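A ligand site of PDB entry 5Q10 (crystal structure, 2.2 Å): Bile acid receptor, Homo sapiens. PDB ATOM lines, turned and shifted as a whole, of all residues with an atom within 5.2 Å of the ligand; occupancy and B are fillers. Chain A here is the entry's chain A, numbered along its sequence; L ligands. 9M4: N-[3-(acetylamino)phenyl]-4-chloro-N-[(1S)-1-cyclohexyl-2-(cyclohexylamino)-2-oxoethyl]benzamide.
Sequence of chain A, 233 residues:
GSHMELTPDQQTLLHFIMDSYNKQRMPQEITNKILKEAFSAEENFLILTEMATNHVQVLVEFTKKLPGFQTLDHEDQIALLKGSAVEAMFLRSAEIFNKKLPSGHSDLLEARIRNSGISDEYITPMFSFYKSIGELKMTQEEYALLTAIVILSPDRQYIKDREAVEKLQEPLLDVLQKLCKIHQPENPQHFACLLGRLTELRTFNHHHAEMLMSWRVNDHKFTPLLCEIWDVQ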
ATOM      1  N   PHE A  45      19.231  -2.761 -22.569  1.00  0.00           N
ATOM      2  CA  PHE A  45      19.369  -4.099 -21.995  1.00  0.00           C
ATOM      3  C   PHE A  45      19.511  -5.143 -23.091  1.00  0.00           C
ATOM      4  O   PHE A  45      20.294  -6.085 -22.953  1.00  0.00           O
ATOM      5  CB  PHE A  45      18.194  -4.411 -21.076  1.00  0.00           C
ATOM      6  CG  PHE A  45      18.471  -5.585 -20.169  1.00  0.00           C
ATOM      7  CD1 PHE A  45      19.241  -5.444 -19.024  1.00  0.00           C
ATOM      8  CD2 PHE A  45      17.964  -6.849 -20.480  1.00  0.00           C
ATOM      9  CE1 PHE A  45      19.522  -6.531 -18.213  1.00  0.00           C
ATOM     10  CE2 PHE A  45      18.243  -7.945 -19.658  1.00  0.00           C
ATOM     11  CZ  PHE A  45      19.011  -7.771 -18.525  1.00  0.00           C
ATOM     12  N   LEU A  48      23.100  -5.142 -24.343  1.00  0.00           N
ATOM     13  CA  LEU A  48      23.960  -5.844 -23.383  1.00  0.00           C
ATOM     14  C   LEU A  48      23.753  -7.355 -23.433  1.00  0.00           C
ATOM     15  O   LEU A  48      24.683  -8.102 -23.150  1.00  0.00           O
ATOM     16  CB  LEU A  48      23.785  -5.316 -21.949  1.00  0.00           C
ATOM     17  CG  LEU A  48      24.017  -3.810 -21.708  1.00  0.00           C
ATOM     18  CD1 LEU A  48      23.936  -3.481 -20.226  1.00  0.00           C
ATOM     19  CD2 LEU A  48      25.344  -3.348 -22.281  1.00  0.00           C
ATOM     20  N   THR A  49      22.541  -7.810 -23.791  1.00  0.00           N
ATOM     21  CA  THR A  49      22.189  -9.230 -23.955  1.00  0.00           C
ATOM     22  C   THR A  49      22.966  -9.748 -25.170  1.00  0.00           C
ATOM     23  O   THR A  49      23.582 -10.806 -25.076  1.00  0.00           O
ATOM     24  CB  THR A  49      20.663  -9.391 -24.086  1.00  0.00           C
ATOM     25  OG1 THR A  49      20.046  -8.808 -22.936  1.00  0.00           O
ATOM     26  CG2 THR A  49      20.234 -10.841 -24.201  1.00  0.00           C
ATOM     27  N   MET A  51      25.755  -8.510 -26.394  1.00  0.00           N
ATOM     28  CA  MET A  51      27.165  -8.491 -26.019  1.00  0.00           C
ATOM     29  C   MET A  51      27.535  -9.700 -25.168  1.00  0.00           C
ATOM     30  O   MET A  51      28.576 -10.302 -25.404  1.00  0.00           O
ATOM     31  CB  MET A  51      27.548  -7.166 -25.346  1.00  0.00           C
ATOM     32  CG  MET A  51      27.385  -5.974 -26.256  1.00  0.00           C
ATOM     33  SD  MET A  51      27.922  -4.420 -25.529  1.00  0.00           S
ATOM     34  CE  MET A  51      29.687  -4.518 -25.823  1.00  0.00           C
ATOM     35  N   ALA A  52      26.658 -10.081 -24.235  1.00  0.00           N
ATOM     36  CA  ALA A  52      26.825 -11.262 -23.360  1.00  0.00           C
ATOM     37  C   ALA A  52      26.840 -12.560 -24.182  1.00  0.00           C
ATOM     38  O   ALA A  52      27.708 -13.398 -23.964  1.00  0.00           O
ATOM     39  CB  ALA A  52      25.697 -11.312 -22.336  1.00  0.00           C
ATOM     40  N   HIS A  55      30.081 -12.750 -26.234  1.00  0.00           N
ATOM     41  CA  HIS A  55      31.191 -13.100 -25.347  1.00  0.00           C
ATOM     42  C   HIS A  55      31.269 -14.620 -25.100  1.00  0.00           C
ATOM     43  O   HIS A  55      32.359 -15.170 -25.178  1.00  0.00           O
ATOM     44  CB  HIS A  55      31.164 -12.312 -24.015  1.00  0.00           C
ATOM     45  CG  HIS A  55      31.916 -13.002 -22.911  1.00  0.00           C
ATOM     46  ND1 HIS A  55      33.302 -13.029 -22.890  1.00  0.00           N
ATOM     47  CD2 HIS A  55      31.454 -13.759 -21.892  1.00  0.00           C
ATOM     48  CE1 HIS A  55      33.634 -13.776 -21.853  1.00  0.00           C
ATOM     49  NE2 HIS A  55      32.548 -14.233 -21.206  1.00  0.00           N
ATOM     50  N   VAL A  56      30.121 -15.271 -24.843  1.00  0.00           N
ATOM     51  CA  VAL A  56      30.066 -16.713 -24.600  1.00  0.00           C
ATOM     52  C   VAL A  56      30.619 -17.491 -25.811  1.00  0.00           C
ATOM     53  O   VAL A  56      31.430 -18.396 -25.629  1.00  0.00           O
ATOM     54  CB  VAL A  56      28.652 -17.191 -24.149  1.00  0.00           C
ATOM     55  CG1 VAL A  56      28.588 -18.712 -24.010  1.00  0.00           C
ATOM     56  CG2 VAL A  56      28.245 -16.524 -22.831  1.00  0.00           C
ATOM     57  N   ALA A  85      33.430 -18.031 -17.172  1.00  0.00           N
ATOM     58  CA  ALA A  85      32.673 -17.165 -18.093  1.00  0.00           C
ATOM     59  C   ALA A  85      32.477 -15.717 -17.635  1.00  0.00           C
ATOM     60  O   ALA A  85      32.640 -14.817 -18.437  1.00  0.00           O
ATOM     61  CB  ALA A  85      31.326 -17.788 -18.447  1.00  0.00           C
ATOM     62  N   VAL A  86      32.119 -15.521 -16.355  1.00  0.00           N
ATOM     63  CA  VAL A  86      31.885 -14.190 -15.778  1.00  0.00           C
ATOM     64  C   VAL A  86      33.185 -13.367 -15.682  1.00  0.00           C
ATOM     65  O   VAL A  86      33.201 -12.207 -16.115  1.00  0.00           O
ATOM     66  CB  VAL A  86      31.113 -14.275 -14.423  1.00  0.00           C
ATOM     67  CG1 VAL A  86      30.999 -12.914 -13.739  1.00  0.00           C
ATOM     68  CG2 VAL A  86      29.737 -14.898 -14.614  1.00  0.00           C
ATOM     69  N   MET A  89      34.450 -12.332 -19.107  1.00  0.00           N
ATOM     70  CA  MET A  89      33.578 -11.277 -19.641  1.00  0.00           C
ATOM     71  C   MET A  89      34.072  -9.924 -19.197  1.00  0.00           C
ATOM     72  O   MET A  89      34.201  -9.037 -20.044  1.00  0.00           O
ATOM     73  CB  MET A  89      32.123 -11.513 -19.184  1.00  0.00           C
ATOM     74  CG  MET A  89      31.116 -10.597 -19.863  1.00  0.00           C
ATOM     75  SD  MET A  89      29.898  -9.907 -18.713  1.00  0.00           S
ATOM     76  CE  MET A  89      30.913  -8.731 -17.866  1.00  0.00           C
ATOM     77  N   PHE A  90      34.378  -9.768 -17.898  1.00  0.00           N
ATOM     78  CA  PHE A  90      34.880  -8.499 -17.352  1.00  0.00           C
ATOM     79  C   PHE A  90      36.232  -8.130 -17.898  1.00  0.00           C
ATOM     80  O   PHE A  90      36.490  -6.950 -18.096  1.00  0.00           O
ATOM     81  CB  PHE A  90      34.864  -8.488 -15.818  1.00  0.00           C
ATOM     82  CG  PHE A  90      33.475  -8.363 -15.259  1.00  0.00           C
ATOM     83  CD1 PHE A  90      32.840  -7.137 -15.189  1.00  0.00           C
ATOM     84  CD2 PHE A  90      32.792  -9.489 -14.797  1.00  0.00           C
ATOM     85  CE1 PHE A  90      31.542  -7.034 -14.668  1.00  0.00           C
ATOM     86  CE2 PHE A  90      31.501  -9.386 -14.292  1.00  0.00           C
ATOM     87  CZ  PHE A  90      30.878  -8.163 -14.229  1.00  0.00           C
ATOM     88  N   SER A  93      35.593  -7.183 -21.637  1.00  0.00           N
ATOM     89  CA  SER A  93      34.845  -5.913 -21.581  1.00  0.00           C
ATOM     90  C   SER A  93      35.758  -4.741 -21.282  1.00  0.00           C
ATOM     91  O   SER A  93      35.556  -3.673 -21.855  1.00  0.00           O
ATOM     92  CB  SER A  93      33.740  -5.965 -20.536  1.00  0.00           C
ATOM     93  OG  SER A  93      32.736  -6.889 -20.918  1.00  0.00           O
ATOM     94  N   LEU A 109      28.297   3.606 -25.096  1.00  0.00           N
ATOM     95  CA  LEU A 109      28.112   2.304 -24.459  1.00  0.00           C
ATOM     96  C   LEU A 109      27.937   2.484 -22.932  1.00  0.00           C
ATOM     97  O   LEU A 109      26.992   1.929 -22.366  1.00  0.00           O
ATOM     98  CB  LEU A 109      29.227   1.301 -24.810  1.00  0.00           C
ATOM     99  CG  LEU A 109      29.101  -0.107 -24.184  1.00  0.00           C
ATOM    100  CD1 LEU A 109      27.769  -0.799 -24.558  1.00  0.00           C
ATOM    101  CD2 LEU A 109      30.276  -0.975 -24.563  1.00  0.00           C
ATOM    102  N   ILE A 113      24.813   1.441 -20.637  1.00  0.00           N
ATOM    103  CA  ILE A 113      24.988   0.588 -19.466  1.00  0.00           C
ATOM    104  C   ILE A 113      24.333   1.247 -18.243  1.00  0.00           C
ATOM    105  O   ILE A 113      23.516   0.608 -17.565  1.00  0.00           O
ATOM    106  CB  ILE A 113      26.476   0.218 -19.242  1.00  0.00           C
ATOM    107  CG1 ILE A 113      26.972  -0.736 -20.355  1.00  0.00           C
ATOM    108  CG2 ILE A 113      26.723  -0.382 -17.850  1.00  0.00           C
ATOM    109  CD1 ILE A 113      28.488  -0.864 -20.482  1.00  0.00           C
ATOM    110  N   ILE A 118      19.696  -1.706 -14.811  1.00  0.00           N
ATOM    111  CA  ILE A 118      20.534  -2.403 -13.835  1.00  0.00           C
ATOM    112  C   ILE A 118      20.931  -1.412 -12.732  1.00  0.00           C
ATOM    113  O   ILE A 118      21.338  -0.285 -13.038  1.00  0.00           O
ATOM    114  CB  ILE A 118      21.778  -3.088 -14.501  1.00  0.00           C
ATOM    115  CG1 ILE A 118      21.327  -4.077 -15.607  1.00  0.00           C
ATOM    116  CG2 ILE A 118      22.657  -3.802 -13.446  1.00  0.00           C
ATOM    117  CD1 ILE A 118      22.392  -4.448 -16.633  1.00  0.00           C
ATOM    118  N   TYR A 122      25.684  -2.893  -9.281  1.00  0.00           N
ATOM    119  CA  TYR A 122      26.257  -3.805 -10.280  1.00  0.00           C
ATOM    120  C   TYR A 122      26.912  -3.082 -11.465  1.00  0.00           C
ATOM    121  O   TYR A 122      27.411  -3.752 -12.378  1.00  0.00           O
ATOM    122  CB  TYR A 122      25.204  -4.814 -10.746  1.00  0.00           C
ATOM    123  CG  TYR A 122      24.462  -5.490  -9.602  1.00  0.00           C
ATOM    124  CD1 TYR A 122      23.098  -5.275  -9.417  1.00  0.00           C
ATOM    125  CD2 TYR A 122      25.135  -6.273  -8.675  1.00  0.00           C
ATOM    126  CE1 TYR A 122      22.415  -5.881  -8.360  1.00  0.00           C
ATOM    127  CE2 TYR A 122      24.462  -6.869  -7.608  1.00  0.00           C
ATOM    128  CZ  TYR A 122      23.103  -6.680  -7.459  1.00  0.00           C
ATOM    129  OH  TYR A 122      22.446  -7.283  -6.428  1.00  0.00           O
ATOM    130  N   ILE A 123      26.946  -1.724 -11.444  1.00  0.00           N
ATOM    131  CA  ILE A 123      27.540  -0.875 -12.490  1.00  0.00           C
ATOM    132  C   ILE A 123      28.856  -0.225 -11.998  1.00  0.00           C
ATOM    133  O   ILE A 123      29.824  -0.202 -12.751  1.00  0.00           O
ATOM    134  CB  ILE A 123      26.505   0.199 -13.016  1.00  0.00           C
ATOM    135  CG1 ILE A 123      25.167  -0.422 -13.509  1.00  0.00           C
ATOM    136  CG2 ILE A 123      27.098   1.125 -14.085  1.00  0.00           C
ATOM    137  CD1 ILE A 123      25.211  -1.399 -14.706  1.00  0.00           C
ATOM    138  N   MET A 126      32.245  -2.333 -11.726  1.00  0.00           N
ATOM    139  CA  MET A 126      32.571  -2.621 -13.125  1.00  0.00           C
ATOM    140  C   MET A 126      33.419  -1.501 -13.738  1.00  0.00           C
ATOM    141  O   MET A 126      34.500  -1.781 -14.283  1.00  0.00           O
ATOM    142  CB  MET A 126      31.261  -2.899 -13.888  1.00  0.00           C
ATOM    143  CG  MET A 126      31.306  -2.614 -15.367  1.00  0.00           C
ATOM    144  SD  MET A 126      29.707  -3.022 -16.118  1.00  0.00           S
ATOM    145  CE  MET A 126      29.957  -4.696 -16.415  1.00  0.00           C
ATOM    146  N   TYR A 130      37.548  -1.211 -14.715  1.00  0.00           N
ATOM    147  CA  TYR A 130      38.030  -0.746 -16.025  1.00  0.00           C
ATOM    148  C   TYR A 130      39.124   0.294 -15.866  1.00  0.00           C
ATOM    149  O   TYR A 130      40.122   0.221 -16.584  1.00  0.00           O
ATOM    150  CB  TYR A 130      36.899  -0.170 -16.886  1.00  0.00           C
ATOM    151  CG  TYR A 130      35.794  -1.127 -17.291  1.00  0.00           C
ATOM    152  CD1 TYR A 130      35.968  -2.505 -17.202  1.00  0.00           C
ATOM    153  CD2 TYR A 130      34.595  -0.647 -17.801  1.00  0.00           C
ATOM    154  CE1 TYR A 130      34.952  -3.389 -17.576  1.00  0.00           C
ATOM    155  CE2 TYR A 130      33.576  -1.521 -18.194  1.00  0.00           C
ATOM    156  CZ  TYR A 130      33.764  -2.890 -18.087  1.00  0.00           C
ATOM    157  OH  TYR A 130      32.761  -3.731 -18.480  1.00  0.00           O
ATOM    158  N   PHE A 204      33.671 -10.332  -8.677  1.00  0.00           N
ATOM    159  CA  PHE A 204      32.571 -10.113  -9.612  1.00  0.00           C
ATOM    160  C   PHE A 204      31.642 -11.301  -9.713  1.00  0.00           C
ATOM    161  O   PHE A 204      30.478 -11.110 -10.096  1.00  0.00           O
ATOM    162  CB  PHE A 204      33.071  -9.658 -10.997  1.00  0.00           C
ATOM    163  CG  PHE A 204      33.570  -8.241 -10.960  1.00  0.00           C
ATOM    164  CD1 PHE A 204      34.934  -7.962 -10.899  1.00  0.00           C
ATOM    165  CD2 PHE A 204      32.671  -7.169 -10.925  1.00  0.00           C
ATOM    166  CE1 PHE A 204      35.392  -6.637 -10.806  1.00  0.00           C
ATOM    167  CE2 PHE A 204      33.135  -5.844 -10.849  1.00  0.00           C
ATOM    168  CZ  PHE A 204      34.485  -5.592 -10.775  1.00  0.00           C
ATOM    169  N   HIS A 207      28.955 -10.705  -6.968  1.00  0.00           N
ATOM    170  CA  HIS A 207      28.184  -9.527  -7.378  1.00  0.00           C
ATOM    171  C   HIS A 207      27.218  -9.950  -8.483  1.00  0.00           C
ATOM    172  O   HIS A 207      26.033  -9.631  -8.410  1.00  0.00           O
ATOM    173  CB  HIS A 207      29.092  -8.398  -7.916  1.00  0.00           C
ATOM    174  CG  HIS A 207      29.835  -7.606  -6.882  1.00  0.00           C
ATOM    175  ND1 HIS A 207      31.019  -6.960  -7.186  1.00  0.00           N
ATOM    176  CD2 HIS A 207      29.522  -7.360  -5.590  1.00  0.00           C
ATOM    177  CE1 HIS A 207      31.404  -6.362  -6.071  1.00  0.00           C
ATOM    178  NE2 HIS A 207      30.543  -6.570  -5.079  1.00  0.00           N
ATOM    179  N   HIS A 208      27.733 -10.678  -9.496  1.00  0.00           N
ATOM    180  CA  HIS A 208      27.000 -11.171 -10.658  1.00  0.00           C
ATOM    181  C   HIS A 208      25.858 -12.130 -10.286  1.00  0.00           C
ATOM    182  O   HIS A 208      24.753 -11.975 -10.814  1.00  0.00           O
ATOM    183  CB  HIS A 208      27.976 -11.848 -11.645  1.00  0.00           C
ATOM    184  CG  HIS A 208      27.325 -12.339 -12.891  1.00  0.00           C
ATOM    185  ND1 HIS A 208      26.892 -13.644 -13.017  1.00  0.00           N
ATOM    186  CD2 HIS A 208      27.043 -11.676 -14.022  1.00  0.00           C
ATOM    187  CE1 HIS A 208      26.378 -13.743 -14.219  1.00  0.00           C
ATOM    188  NE2 HIS A 208      26.433 -12.572 -14.867  1.00  0.00           N
ATOM    189  N   MET A 211      23.117 -10.254  -8.573  1.00  0.00           N
ATOM    190  CA  MET A 211      22.415  -9.513  -9.618  1.00  0.00           C
ATOM    191  C   MET A 211      21.389 -10.396 -10.351  1.00  0.00           C
ATOM    192  O   MET A 211      20.249  -9.972 -10.539  1.00  0.00           O
ATOM    193  CB  MET A 211      23.421  -8.888 -10.599  1.00  0.00           C
ATOM    194  CG  MET A 211      22.781  -8.111 -11.718  1.00  0.00           C
ATOM    195  SD  MET A 211      23.967  -7.653 -13.010  1.00  0.00           S
ATOM    196  CE  MET A 211      24.255  -9.261 -13.796  1.00  0.00           C
ATOM    197  N   LEU A 212      21.803 -11.622 -10.736  1.00  0.00           N
ATOM    198  CA  LEU A 212      20.926 -12.570 -11.434  1.00  0.00           C
ATOM    199  C   LEU A 212      19.778 -13.091 -10.564  1.00  0.00           C
ATOM    200  O   LEU A 212      18.649 -13.188 -11.050  1.00  0.00           O
ATOM    201  CB  LEU A 212      21.716 -13.744 -12.044  1.00  0.00           C
ATOM    202  CG  LEU A 212      22.727 -13.452 -13.161  1.00  0.00           C
ATOM    203  CD1 LEU A 212      23.136 -14.733 -13.829  1.00  0.00           C
ATOM    204  CD2 LEU A 212      22.150 -12.521 -14.233  1.00  0.00           C
ATOM    205  N   TRP A 215      16.725 -10.798 -10.385  1.00  0.00           N
ATOM    206  CA  TRP A 215      15.925 -10.688 -11.613  1.00  0.00           C
ATOM    207  C   TRP A 215      14.846 -11.777 -11.723  1.00  0.00           C
ATOM    208  O   TRP A 215      13.993 -11.693 -12.598  1.00  0.00           O
ATOM    209  CB  TRP A 215      16.829 -10.716 -12.866  1.00  0.00           C
ATOM    210  CG  TRP A 215      17.808  -9.583 -13.008  1.00  0.00           C
ATOM    211  CD1 TRP A 215      17.914  -8.465 -12.233  1.00  0.00           C
ATOM    212  CD2 TRP A 215      18.825  -9.458 -14.013  1.00  0.00           C
ATOM    213  NE1 TRP A 215      18.932  -7.660 -12.677  1.00  0.00           N
ATOM    214  CE2 TRP A 215      19.514  -8.254 -13.773  1.00  0.00           C
ATOM    215  CE3 TRP A 215      19.231 -10.270 -15.097  1.00  0.00           C
ATOM    216  CZ2 TRP A 215      20.584  -7.823 -14.576  1.00  0.00           C
ATOM    217  CZ3 TRP A 215      20.287  -9.844 -15.882  1.00  0.00           C
ATOM    218  CH2 TRP A 215      20.957  -8.638 -15.618  1.00  0.00           C
ATOM    219  N   LYS A 221      14.182  -7.942 -17.314  1.00  0.00           N
ATOM    220  CA  LYS A 221      15.599  -8.318 -17.218  1.00  0.00           C
ATOM    221  C   LYS A 221      15.880  -9.830 -17.300  1.00  0.00           C
ATOM    222  O   LYS A 221      16.995 -10.205 -17.664  1.00  0.00           O
ATOM    223  CB  LYS A 221      16.244  -7.707 -15.965  1.00  0.00           C
ATOM    224  CG  LYS A 221      16.518  -6.211 -16.106  1.00  0.00           C
ATOM    225  CD  LYS A 221      17.222  -5.612 -14.893  1.00  0.00           C
ATOM    226  CE  LYS A 221      16.264  -5.106 -13.839  1.00  0.00           C
ATOM    227  NZ  LYS A 221      16.983  -4.576 -12.646  1.00  0.00           N
ATOM    228  N   THR A 223      16.557 -13.193 -18.640  1.00  0.00           N
ATOM    229  CA  THR A 223      17.010 -13.785 -19.900  1.00  0.00           C
ATOM    230  C   THR A 223      17.293 -15.293 -19.701  1.00  0.00           C
ATOM    231  O   THR A 223      18.375 -15.665 -19.231  1.00  0.00           O
ATOM    232  CB  THR A 223      18.170 -12.967 -20.523  1.00  0.00           C
ATOM    233  OG1 THR A 223      18.646 -13.637 -21.701  1.00  0.00           O
ATOM    234  CG2 THR A 223      19.311 -12.734 -19.550  1.00  0.00           C
ATOM    235  N   LEU A 226      20.990 -17.221 -20.677  1.00  0.00           N
ATOM    236  CA  LEU A 226      22.141 -17.022 -19.806  1.00  0.00           C
ATOM    237  C   LEU A 226      21.849 -17.365 -18.342  1.00  0.00           C
ATOM    238  O   LEU A 226      22.696 -17.981 -17.697  1.00  0.00           O
ATOM    239  CB  LEU A 226      22.702 -15.596 -19.963  1.00  0.00           C
ATOM    240  CG  LEU A 226      23.251 -15.258 -21.366  1.00  0.00           C
ATOM    241  CD1 LEU A 226      23.025 -13.814 -21.706  1.00  0.00           C
ATOM    242  CD2 LEU A 226      24.725 -15.645 -21.516  1.00  0.00           C
ATOM    243  N   TRP A 230      24.139 -19.606 -15.570  1.00  0.00           N
ATOM    244  CA  TRP A 230      24.748 -18.758 -14.546  1.00  0.00           C
ATOM    245  C   TRP A 230      23.718 -18.161 -13.613  1.00  0.00           C
ATOM    246  O   TRP A 230      23.741 -18.463 -12.425  1.00  0.00           O
ATOM    247  CB  TRP A 230      25.603 -17.677 -15.212  1.00  0.00           C
ATOM    248  CG  TRP A 230      26.712 -18.244 -16.050  1.00  0.00           C
ATOM    249  CD1 TRP A 230      27.920 -18.681 -15.604  1.00  0.00           C
ATOM    250  CD2 TRP A 230      26.657 -18.536 -17.449  1.00  0.00           C
ATOM    251  NE1 TRP A 230      28.653 -19.193 -16.656  1.00  0.00           N
ATOM    252  CE2 TRP A 230      27.895 -19.115 -17.798  1.00  0.00           C
ATOM    253  CE3 TRP A 230      25.702 -18.343 -18.457  1.00  0.00           C
ATOM    254  CZ2 TRP A 230      28.196 -19.520 -19.110  1.00  0.00           C
ATOM    255  CZ3 TRP A 230      25.993 -18.740 -19.749  1.00  0.00           C
ATOM    256  CH2 TRP A 230      27.234 -19.308 -20.072  1.00  0.00           C
HETATM  257  C4  9M4 L   1      29.779  -5.467 -19.744  1.00  0.00           C
HETATM  258  C5  9M4 L   1      29.544  -4.871 -20.975  1.00  0.00           C
HETATM  259  C6  9M4 L   1      28.514  -5.286 -21.795  1.00  0.00           C
HETATM  260  C7  9M4 L   1      27.694  -6.312 -21.375  1.00  0.00           C
HETATM  261  C10 9M4 L   1      25.327  -9.109 -18.157  1.00  0.00           C
HETATM  262  C15 9M4 L   1      27.173 -12.514 -18.486  1.00  0.00           C
HETATM  263  C17 9M4 L   1      27.027 -14.954 -17.843  1.00  0.00           C
HETATM  264  C20 9M4 L   1      28.070 -12.857 -19.667  1.00  0.00           C
HETATM  265  C21 9M4 L   1      23.290 -10.533 -18.644  1.00  0.00           C
HETATM  266  C22 9M4 L   1      22.209 -10.853 -19.657  1.00  0.00           C
HETATM  267  C24 9M4 L   1      22.177  -8.410 -20.360  1.00  0.00           C
HETATM  268  C26 9M4 L   1      26.280  -6.861 -17.640  1.00  0.00           C
HETATM  269  C28 9M4 L   1      26.748  -6.005 -15.420  1.00  0.00           C
HETATM  270  C1  9M4 L   1      26.983  -8.068 -19.727  1.00  0.00           C
HETATM  271  O32 9M4 L   1      26.903  -9.036 -20.457  1.00  0.00           O
HETATM  272  C2  9M4 L   1      27.893  -6.944 -20.134  1.00  0.00           C
HETATM  273  C3  9M4 L   1      28.950  -6.505 -19.334  1.00  0.00           C
HETATM  274 CL8  9M4 L   1      30.587  -3.578 -21.493  1.00  0.00          CL
HETATM  275  N9  9M4 L   1      26.232  -7.980 -18.535  1.00  0.00           N
HETATM  276  C11 9M4 L   1      24.195  -9.395 -19.140  1.00  0.00           C
HETATM  277  C23 9M4 L   1      21.324  -9.643 -19.939  1.00  0.00           C
HETATM  278  C25 9M4 L   1      23.338  -8.147 -19.378  1.00  0.00           C
HETATM  279  C12 9M4 L   1      26.156 -10.372 -17.750  1.00  0.00           C
HETATM  280  O13 9M4 L   1      26.554 -10.499 -16.599  1.00  0.00           O
HETATM  281  N14 9M4 L   1      26.404 -11.279 -18.719  1.00  0.00           N
HETATM  282  C16 9M4 L   1      26.235 -13.678 -18.160  1.00  0.00           C
HETATM  283  C18 9M4 L   1      27.964 -15.336 -18.989  1.00  0.00           C
HETATM  284  C19 9M4 L   1      28.887 -14.150 -19.384  1.00  0.00           C
HETATM  285  C27 9M4 L   1      26.686  -7.068 -16.313  1.00  0.00           C
HETATM  286  C29 9M4 L   1      26.387  -4.731 -15.855  1.00  0.00           C
HETATM  287  C30 9M4 L   1      25.975  -4.525 -17.165  1.00  0.00           C
HETATM  288  C31 9M4 L   1      25.921  -5.582 -18.061  1.00  0.00           C
HETATM  289  N33 9M4 L   1      27.163  -6.180 -14.077  1.00  0.00           N
HETATM  290  C34 9M4 L   1      27.558  -7.322 -13.438  1.00  0.00           C
HETATM  291  O36 9M4 L   1      27.619  -8.411 -13.989  1.00  0.00           O
HETATM  292  C35 9M4 L   1      27.932  -7.148 -11.992  1.00  0.00           C
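Merely in contact with the ligand: Ala 52, Phe 90, Phe 45, Thr 49, Met 126, Thr 223, Ser 93, Ile 113, His 55, Leu 48, Trp 230, Ile 118, Tyr 130, Leu 226, Ile 123, Met 51 and Ala 85. Of the 29 residues printed, 21 come within 4 Å of the ligand. Along chain A the residues within 4 Å of the ligand span positions 45 to 230.
An oxygen (O13) of the ligand sits at hydrogen-bond distance from a ring nitrogen (NE2) of His 208, 2.7 Å away. O of Tyr 122 sits at hydrogen-bond distance from N33 of the ligand (3.0 Å). A nitrogen (N14) of the ligand lies close to the side-chain sulfur (SD) of Met 89, 3.8 Å away. The side-chain sulfur of Met 211 lies close to a nitrogen (N33) of the ligand.
The side-chain hydroxyl (OG1) of Thr 49 is in hydrogen-bond range of the backbone carbonyl oxygen (O) of Phe 45 (2.7 Å). The backbone carbonyl oxygen of Met 89 is in hydrogen-bond range of the side-chain hydroxyl of Ser 93 (2.7 Å). The backbone NH (N) of Met 89 lies close to a ring nitrogen (NE2) of His 55 (3.4 Å). The indole nitrogen (NE1) of Trp 215 lies close to the backbone carbonyl oxygen (O) of Met 211, 3.4 Å away. The backbone carbonyl oxygen (O) of Ala 85 is in hydrogen-bond range of a ring nitrogen (NE2) of His 55, at 2.8 Å.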
